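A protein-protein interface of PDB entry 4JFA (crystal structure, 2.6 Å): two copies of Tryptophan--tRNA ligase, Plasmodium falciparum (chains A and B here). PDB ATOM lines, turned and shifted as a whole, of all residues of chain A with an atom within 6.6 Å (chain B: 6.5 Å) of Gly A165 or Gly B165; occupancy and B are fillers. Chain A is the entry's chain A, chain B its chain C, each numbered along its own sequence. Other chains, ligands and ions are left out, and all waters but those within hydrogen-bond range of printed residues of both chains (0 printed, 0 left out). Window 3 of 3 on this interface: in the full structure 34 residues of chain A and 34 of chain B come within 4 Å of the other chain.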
ATOM      1  N   ASN A 160      17.021 -37.772  -6.900  1.00  0.00           N
ATOM      2  CA  ASN A 160      16.330 -36.650  -6.275  1.00  0.00           C
ATOM      3  C   ASN A 160      17.230 -35.924  -5.281  1.00  0.00           C
ATOM      4  O   ASN A 160      17.203 -34.696  -5.186  1.00  0.00           O
ATOM      5  CB  ASN A 160      15.042 -37.113  -5.589  1.00  0.00           C
ATOM      6  CG  ASN A 160      13.936 -37.440  -6.578  1.00  0.00           C
ATOM      7  OD1 ASN A 160      14.001 -37.064  -7.750  1.00  0.00           O
ATOM      8  ND2 ASN A 160      12.905 -38.134  -6.104  1.00  0.00           N
ATOM      9  N   THR A 161      18.044 -36.693  -4.561  1.00  0.00           N
ATOM     10  CA  THR A 161      19.006 -36.138  -3.609  1.00  0.00           C
ATOM     11  C   THR A 161      20.032 -35.209  -4.266  1.00  0.00           C
ATOM     12  O   THR A 161      20.700 -34.436  -3.577  1.00  0.00           O
ATOM     13  CB  THR A 161      19.756 -37.247  -2.837  1.00  0.00           C
ATOM     14  OG1 THR A 161      20.257 -38.224  -3.759  1.00  0.00           O
ATOM     15  CG2 THR A 161      18.828 -37.922  -1.840  1.00  0.00           C
ATOM     16  N   GLU A 162      20.155 -35.289  -5.589  1.00  0.00           N
ATOM     17  CA  GLU A 162      21.111 -34.468  -6.330  1.00  0.00           C
ATOM     18  C   GLU A 162      20.433 -33.440  -7.241  1.00  0.00           C
ATOM     19  O   GLU A 162      21.040 -32.432  -7.605  1.00  0.00           O
ATOM     20  CB  GLU A 162      22.045 -35.355  -7.167  1.00  0.00           C
ATOM     21  CG  GLU A 162      22.886 -36.348  -6.367  1.00  0.00           C
ATOM     22  CD  GLU A 162      23.822 -37.172  -7.244  1.00  0.00           C
ATOM     23  OE1 GLU A 162      23.517 -37.356  -8.444  1.00  0.00           O
ATOM     24  OE2 GLU A 162      24.860 -37.640  -6.733  1.00  0.00           O
ATOM     25  N   TYR A 163      19.176 -33.695  -7.599  1.00  0.00           N
ATOM     26  CA  TYR A 163      18.477 -32.913  -8.624  1.00  0.00           C
ATOM     27  C   TYR A 163      17.307 -32.105  -8.046  1.00  0.00           C
ATOM     28  O   TYR A 163      16.585 -31.388  -8.773  1.00  0.00           O
ATOM     29  CB  TYR A 163      17.984 -33.857  -9.723  1.00  0.00           C
ATOM     30  CG  TYR A 163      17.714 -33.192 -11.050  1.00  0.00           C
ATOM     31  CD1 TYR A 163      18.748 -32.641 -11.792  1.00  0.00           C
ATOM     32  CD2 TYR A 163      16.432 -33.135 -11.571  1.00  0.00           C
ATOM     33  CE1 TYR A 163      18.508 -32.035 -13.010  1.00  0.00           C
ATOM     34  CE2 TYR A 163      16.182 -32.532 -12.789  1.00  0.00           C
ATOM     35  CZ  TYR A 163      17.225 -31.983 -13.503  1.00  0.00           C
ATOM     36  OH  TYR A 163      16.986 -31.381 -14.716  1.00  0.00           O
ATOM     37  N   ALA A 164      17.129 -32.228  -6.732  1.00  0.00           N
ATOM     38  CA  ALA A 164      16.062 -31.536  -6.019  1.00  0.00           C
ATOM     39  C   ALA A 164      16.082 -30.028  -6.249  1.00  0.00           C
ATOM     40  O   ALA A 164      15.034 -29.391  -6.264  1.00  0.00           O
ATOM     41  CB  ALA A 164      16.144 -31.826  -4.540  1.00  0.00           C
ATOM     42  N   GLY A 165      17.274 -29.461  -6.416  1.00  0.00           N
ATOM     43  CA  GLY A 165      17.408 -28.036  -6.663  1.00  0.00           C
ATOM     44  C   GLY A 165      16.813 -27.647  -8.003  1.00  0.00           C
ATOM     45  O   GLY A 165      16.313 -26.532  -8.176  1.00  0.00           O
ATOM     46  N   TYR A 166      16.875 -28.571  -8.956  1.00  0.00           N
ATOM     47  CA  TYR A 166      16.277 -28.357 -10.264  1.00  0.00           C
ATOM     48  C   TYR A 166      14.784 -28.635 -10.211  1.00  0.00           C
ATOM     49  O   TYR A 166      14.015 -28.092 -11.008  1.00  0.00           O
ATOM     50  CB  TYR A 166      16.939 -29.258 -11.308  1.00  0.00           C
ATOM     51  CG  TYR A 166      18.305 -28.783 -11.740  1.00  0.00           C
ATOM     52  CD1 TYR A 166      18.469 -28.066 -12.917  1.00  0.00           C
ATOM     53  CD2 TYR A 166      19.431 -29.046 -10.974  1.00  0.00           C
ATOM     54  CE1 TYR A 166      19.714 -27.628 -13.318  1.00  0.00           C
ATOM     55  CE2 TYR A 166      20.679 -28.611 -11.365  1.00  0.00           C
ATOM     56  CZ  TYR A 166      20.814 -27.902 -12.538  1.00  0.00           C
ATOM     57  OH  TYR A 166      22.057 -27.466 -12.935  1.00  0.00           O
ATOM     58  N   LEU A 167      14.378 -29.484  -9.273  1.00  0.00           N
ATOM     59  CA  LEU A 167      12.962 -29.821  -9.142  1.00  0.00           C
ATOM     60  C   LEU A 167      12.131 -28.816  -8.326  1.00  0.00           C
ATOM     61  O   LEU A 167      10.916 -28.724  -8.503  1.00  0.00           O
ATOM     62  CB  LEU A 167      12.810 -31.220  -8.543  1.00  0.00           C
ATOM     63  CG  LEU A 167      13.402 -32.356  -9.377  1.00  0.00           C
ATOM     64  CD1 LEU A 167      13.342 -33.676  -8.621  1.00  0.00           C
ATOM     65  CD2 LEU A 167      12.668 -32.461 -10.701  1.00  0.00           C
ATOM     66  N   TYR A 168      12.790 -28.050  -7.462  1.00  0.00           N
ATOM     67  CA  TYR A 168      12.113 -27.352  -6.362  1.00  0.00           C
ATOM     68  C   TYR A 168      11.038 -26.310  -6.719  1.00  0.00           C
ATOM     69  O   TYR A 168       9.950 -26.342  -6.141  1.00  0.00           O
ATOM     70  CB  TYR A 168      13.131 -26.776  -5.364  1.00  0.00           C
ATOM     71  CG  TYR A 168      12.535 -26.445  -4.013  1.00  0.00           C
ATOM     72  CD1 TYR A 168      11.780 -27.380  -3.319  1.00  0.00           C
ATOM     73  CD2 TYR A 168      12.733 -25.202  -3.429  1.00  0.00           C
ATOM     74  CE1 TYR A 168      11.236 -27.086  -2.084  1.00  0.00           C
ATOM     75  CE2 TYR A 168      12.196 -24.901  -2.190  1.00  0.00           C
ATOM     76  CZ  TYR A 168      11.446 -25.845  -1.525  1.00  0.00           C
ATOM     77  OH  TYR A 168      10.907 -25.547  -0.295  1.00  0.00           O
ATOM     78  N   PRO A 169      11.337 -25.376  -7.649  1.00  0.00           N
ATOM     79  CA  PRO A 169      10.297 -24.396  -7.989  1.00  0.00           C
ATOM     80  C   PRO A 169       9.016 -25.045  -8.519  1.00  0.00           C
ATOM     81  O   PRO A 169       7.923 -24.562  -8.214  1.00  0.00           O
ATOM     82  CB  PRO A 169      10.953 -23.559  -9.090  1.00  0.00           C
ATOM     83  CG  PRO A 169      12.417 -23.664  -8.816  1.00  0.00           C
ATOM     84  CD  PRO A 169      12.614 -25.074  -8.327  1.00  0.00           C
ATOM     85  N   ASN B 160      15.867 -19.841  -0.894  1.00  0.00           N
ATOM     86  CA  ASN B 160      15.593 -21.275  -0.849  1.00  0.00           C
ATOM     87  C   ASN B 160      15.301 -21.843  -2.235  1.00  0.00           C
ATOM     88  O   ASN B 160      15.703 -22.967  -2.553  1.00  0.00           O
ATOM     89  CB  ASN B 160      14.447 -21.588   0.117  1.00  0.00           C
ATOM     90  CG  ASN B 160      14.868 -21.489   1.575  1.00  0.00           C
ATOM     91  OD1 ASN B 160      16.057 -21.546   1.895  1.00  0.00           O
ATOM     92  ND2 ASN B 160      13.891 -21.353   2.465  1.00  0.00           N
ATOM     93  N   THR B 161      14.617 -21.051  -3.060  1.00  0.00           N
ATOM     94  CA  THR B 161      14.312 -21.425  -4.442  1.00  0.00           C
ATOM     95  C   THR B 161      15.564 -21.749  -5.255  1.00  0.00           C
ATOM     96  O   THR B 161      15.481 -22.396  -6.298  1.00  0.00           O
ATOM     97  CB  THR B 161      13.518 -20.318  -5.177  1.00  0.00           C
ATOM     98  OG1 THR B 161      14.110 -19.040  -4.907  1.00  0.00           O
ATOM     99  CG2 THR B 161      12.066 -20.307  -4.724  1.00  0.00           C
ATOM    100  N   GLU B 162      16.720 -21.296  -4.773  1.00  0.00           N
ATOM    101  CA  GLU B 162      17.984 -21.491  -5.478  1.00  0.00           C
ATOM    102  C   GLU B 162      18.948 -22.424  -4.740  1.00  0.00           C
ATOM    103  O   GLU B 162      19.832 -23.019  -5.357  1.00  0.00           O
ATOM    104  CB  GLU B 162      18.667 -20.139  -5.728  1.00  0.00           C
ATOM    105  CG  GLU B 162      17.832 -19.147  -6.534  1.00  0.00           C
ATOM    106  CD  GLU B 162      18.547 -17.824  -6.756  1.00  0.00           C
ATOM    107  OE1 GLU B 162      19.595 -17.590  -6.114  1.00  0.00           O
ATOM    108  OE2 GLU B 162      18.059 -17.014  -7.573  1.00  0.00           O
ATOM    109  N   TYR B 163      18.772 -22.553  -3.426  1.00  0.00           N
ATOM    110  CA  TYR B 163      19.732 -23.262  -2.575  1.00  0.00           C
ATOM    111  C   TYR B 163      19.159 -24.575  -2.026  1.00  0.00           C
ATOM    112  O   TYR B 163      19.824 -25.313  -1.270  1.00  0.00           O
ATOM    113  CB  TYR B 163      20.165 -22.345  -1.428  1.00  0.00           C
ATOM    114  CG  TYR B 163      21.508 -22.681  -0.834  1.00  0.00           C
ATOM    115  CD1 TYR B 163      22.675 -22.504  -1.563  1.00  0.00           C
ATOM    116  CD2 TYR B 163      21.613 -23.159   0.463  1.00  0.00           C
ATOM    117  CE1 TYR B 163      23.907 -22.807  -1.022  1.00  0.00           C
ATOM    118  CE2 TYR B 163      22.843 -23.461   1.014  1.00  0.00           C
ATOM    119  CZ  TYR B 163      23.986 -23.285   0.266  1.00  0.00           C
ATOM    120  OH  TYR B 163      25.212 -23.588   0.811  1.00  0.00           O
ATOM    121  N   ALA B 164      17.919 -24.855  -2.419  1.00  0.00           N
ATOM    122  CA  ALA B 164      17.215 -26.059  -1.988  1.00  0.00           C
ATOM    123  C   ALA B 164      18.018 -27.331  -2.230  1.00  0.00           C
ATOM    124  O   ALA B 164      17.955 -28.262  -1.434  1.00  0.00           O
ATOM    125  CB  ALA B 164      15.880 -26.159  -2.675  1.00  0.00           C
ATOM    126  N   GLY B 165      18.764 -27.371  -3.331  1.00  0.00           N
ATOM    127  CA  GLY B 165      19.581 -28.527  -3.652  1.00  0.00           C
ATOM    128  C   GLY B 165      20.690 -28.740  -2.640  1.00  0.00           C
ATOM    129  O   GLY B 165      21.084 -29.875  -2.359  1.00  0.00           O
ATOM    130  N   TYR B 166      21.201 -27.642  -2.093  1.00  0.00           N
ATOM    131  CA  TYR B 166      22.217 -27.715  -1.054  1.00  0.00           C
ATOM    132  C   TYR B 166      21.580 -28.022   0.294  1.00  0.00           C
ATOM    133  O   TYR B 166      22.237 -28.555   1.192  1.00  0.00           O
ATOM    134  CB  TYR B 166      23.003 -26.405  -0.975  1.00  0.00           C
ATOM    135  CG  TYR B 166      23.937 -26.175  -2.142  1.00  0.00           C
ATOM    136  CD1 TYR B 166      25.273 -26.542  -2.070  1.00  0.00           C
ATOM    137  CD2 TYR B 166      23.483 -25.584  -3.314  1.00  0.00           C
ATOM    138  CE1 TYR B 166      26.130 -26.331  -3.134  1.00  0.00           C
ATOM    139  CE2 TYR B 166      24.331 -25.372  -4.381  1.00  0.00           C
ATOM    140  CZ  TYR B 166      25.654 -25.746  -4.286  1.00  0.00           C
ATOM    141  OH  TYR B 166      26.503 -25.535  -5.348  1.00  0.00           O
ATOM    142  N   LEU B 167      20.302 -27.680   0.439  1.00  0.00           N
ATOM    143  CA  LEU B 167      19.605 -27.935   1.703  1.00  0.00           C
ATOM    144  C   LEU B 167      18.974 -29.331   1.831  1.00  0.00           C
ATOM    145  O   LEU B 167      18.703 -29.790   2.939  1.00  0.00           O
ATOM    146  CB  LEU B 167      18.524 -26.880   1.939  1.00  0.00           C
ATOM    147  CG  LEU B 167      18.973 -25.424   2.045  1.00  0.00           C
ATOM    148  CD1 LEU B 167      17.780 -24.519   2.312  1.00  0.00           C
ATOM    149  CD2 LEU B 167      20.014 -25.273   3.137  1.00  0.00           C
ATOM    150  N   TYR B 168      18.760 -30.006   0.706  1.00  0.00           N
ATOM    151  CA  TYR B 168      17.810 -31.123   0.640  1.00  0.00           C
ATOM    152  C   TYR B 168      18.122 -32.392   1.455  1.00  0.00           C
ATOM    153  O   TYR B 168      17.233 -32.896   2.147  1.00  0.00           O
ATOM    154  CB  TYR B 168      17.468 -31.468  -0.817  1.00  0.00           C
ATOM    155  CG  TYR B 168      16.237 -32.329  -0.974  1.00  0.00           C
ATOM    156  CD1 TYR B 168      14.999 -31.895  -0.521  1.00  0.00           C
ATOM    157  CD2 TYR B 168      16.308 -33.571  -1.586  1.00  0.00           C
ATOM    158  CE1 TYR B 168      13.868 -32.679  -0.664  1.00  0.00           C
ATOM    159  CE2 TYR B 168      15.182 -34.359  -1.739  1.00  0.00           C
ATOM    160  CZ  TYR B 168      13.965 -33.909  -1.275  1.00  0.00           C
ATOM    161  OH  TYR B 168      12.843 -34.693  -1.425  1.00  0.00           O
ATOM    162  N   PRO B 169      19.359 -32.924   1.363  1.00  0.00           N
ATOM    163  CA  PRO B 169      19.662 -34.118   2.166  1.00  0.00           C
ATOM    164  C   PRO B 169      19.437 -33.886   3.658  1.00  0.00           C
ATOM    165  O   PRO B 169      18.942 -34.781   4.346  1.00  0.00           O
ATOM    166  CB  PRO B 169      21.150 -34.351   1.899  1.00  0.00           C
ATOM    167  CG  PRO B 169      21.375 -33.778   0.544  1.00  0.00           C
ATOM    168  CD  PRO B 169      20.484 -32.568   0.475  1.00  0.00           C
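Asn A160 touches Tyr B168, and with the chains exchanged Tyr A168 touches Asn B160. Ala A164 touches Tyr B168, and with the chains exchanged Tyr A168 touches Ala B164. Gly A165 touches its own counterpart, Gly B165.
Of chain B, only Gly B165 (3.7 Å) comes within 4 Å of Gly A165. Gly B165 touches just one residue of chain A: Gly A165. Of the printed residues of chain A, Ala B164 touches Tyr A168. Printed residues of chain B within 4 Å of Tyr A168: Asn B160 (3.8 Å) and Ala B164 (3.4 Å). Of the printed residues of chain B, Ala A164 touches Tyr B168 (3.4 Å). Glu A162 touches none of the printed residues of chain B. The nearest residue of chain B that does not touch Gly A165 is Ala B164 (4.5 Å). The nearest printed residue of chain A that does not touch Asn B160 is Gly A165 (6.7 Å).
Among the printed residues, merely in contact across the chains: Tyr A168 with Ala B164 (3.4 Å), Ala A164 with Tyr B168 (3.4 Å), Gly A165 with Gly B165 (3.7 Å), Tyr A168 with Asn B160 (3.8 Å) and Asn A160 with Tyr B168 (3.9 Å).
Hydrophobic or aromatic side chains of chain B that line the printed part of chain A: Ala B164 and Tyr B168. Among the printed residues, 5 pairs touch across the chains. Among the printed residues, no Asp or Glu carboxylate lies within 4 Å of a Lys or Arg side-chain nitrogen of the other chain.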
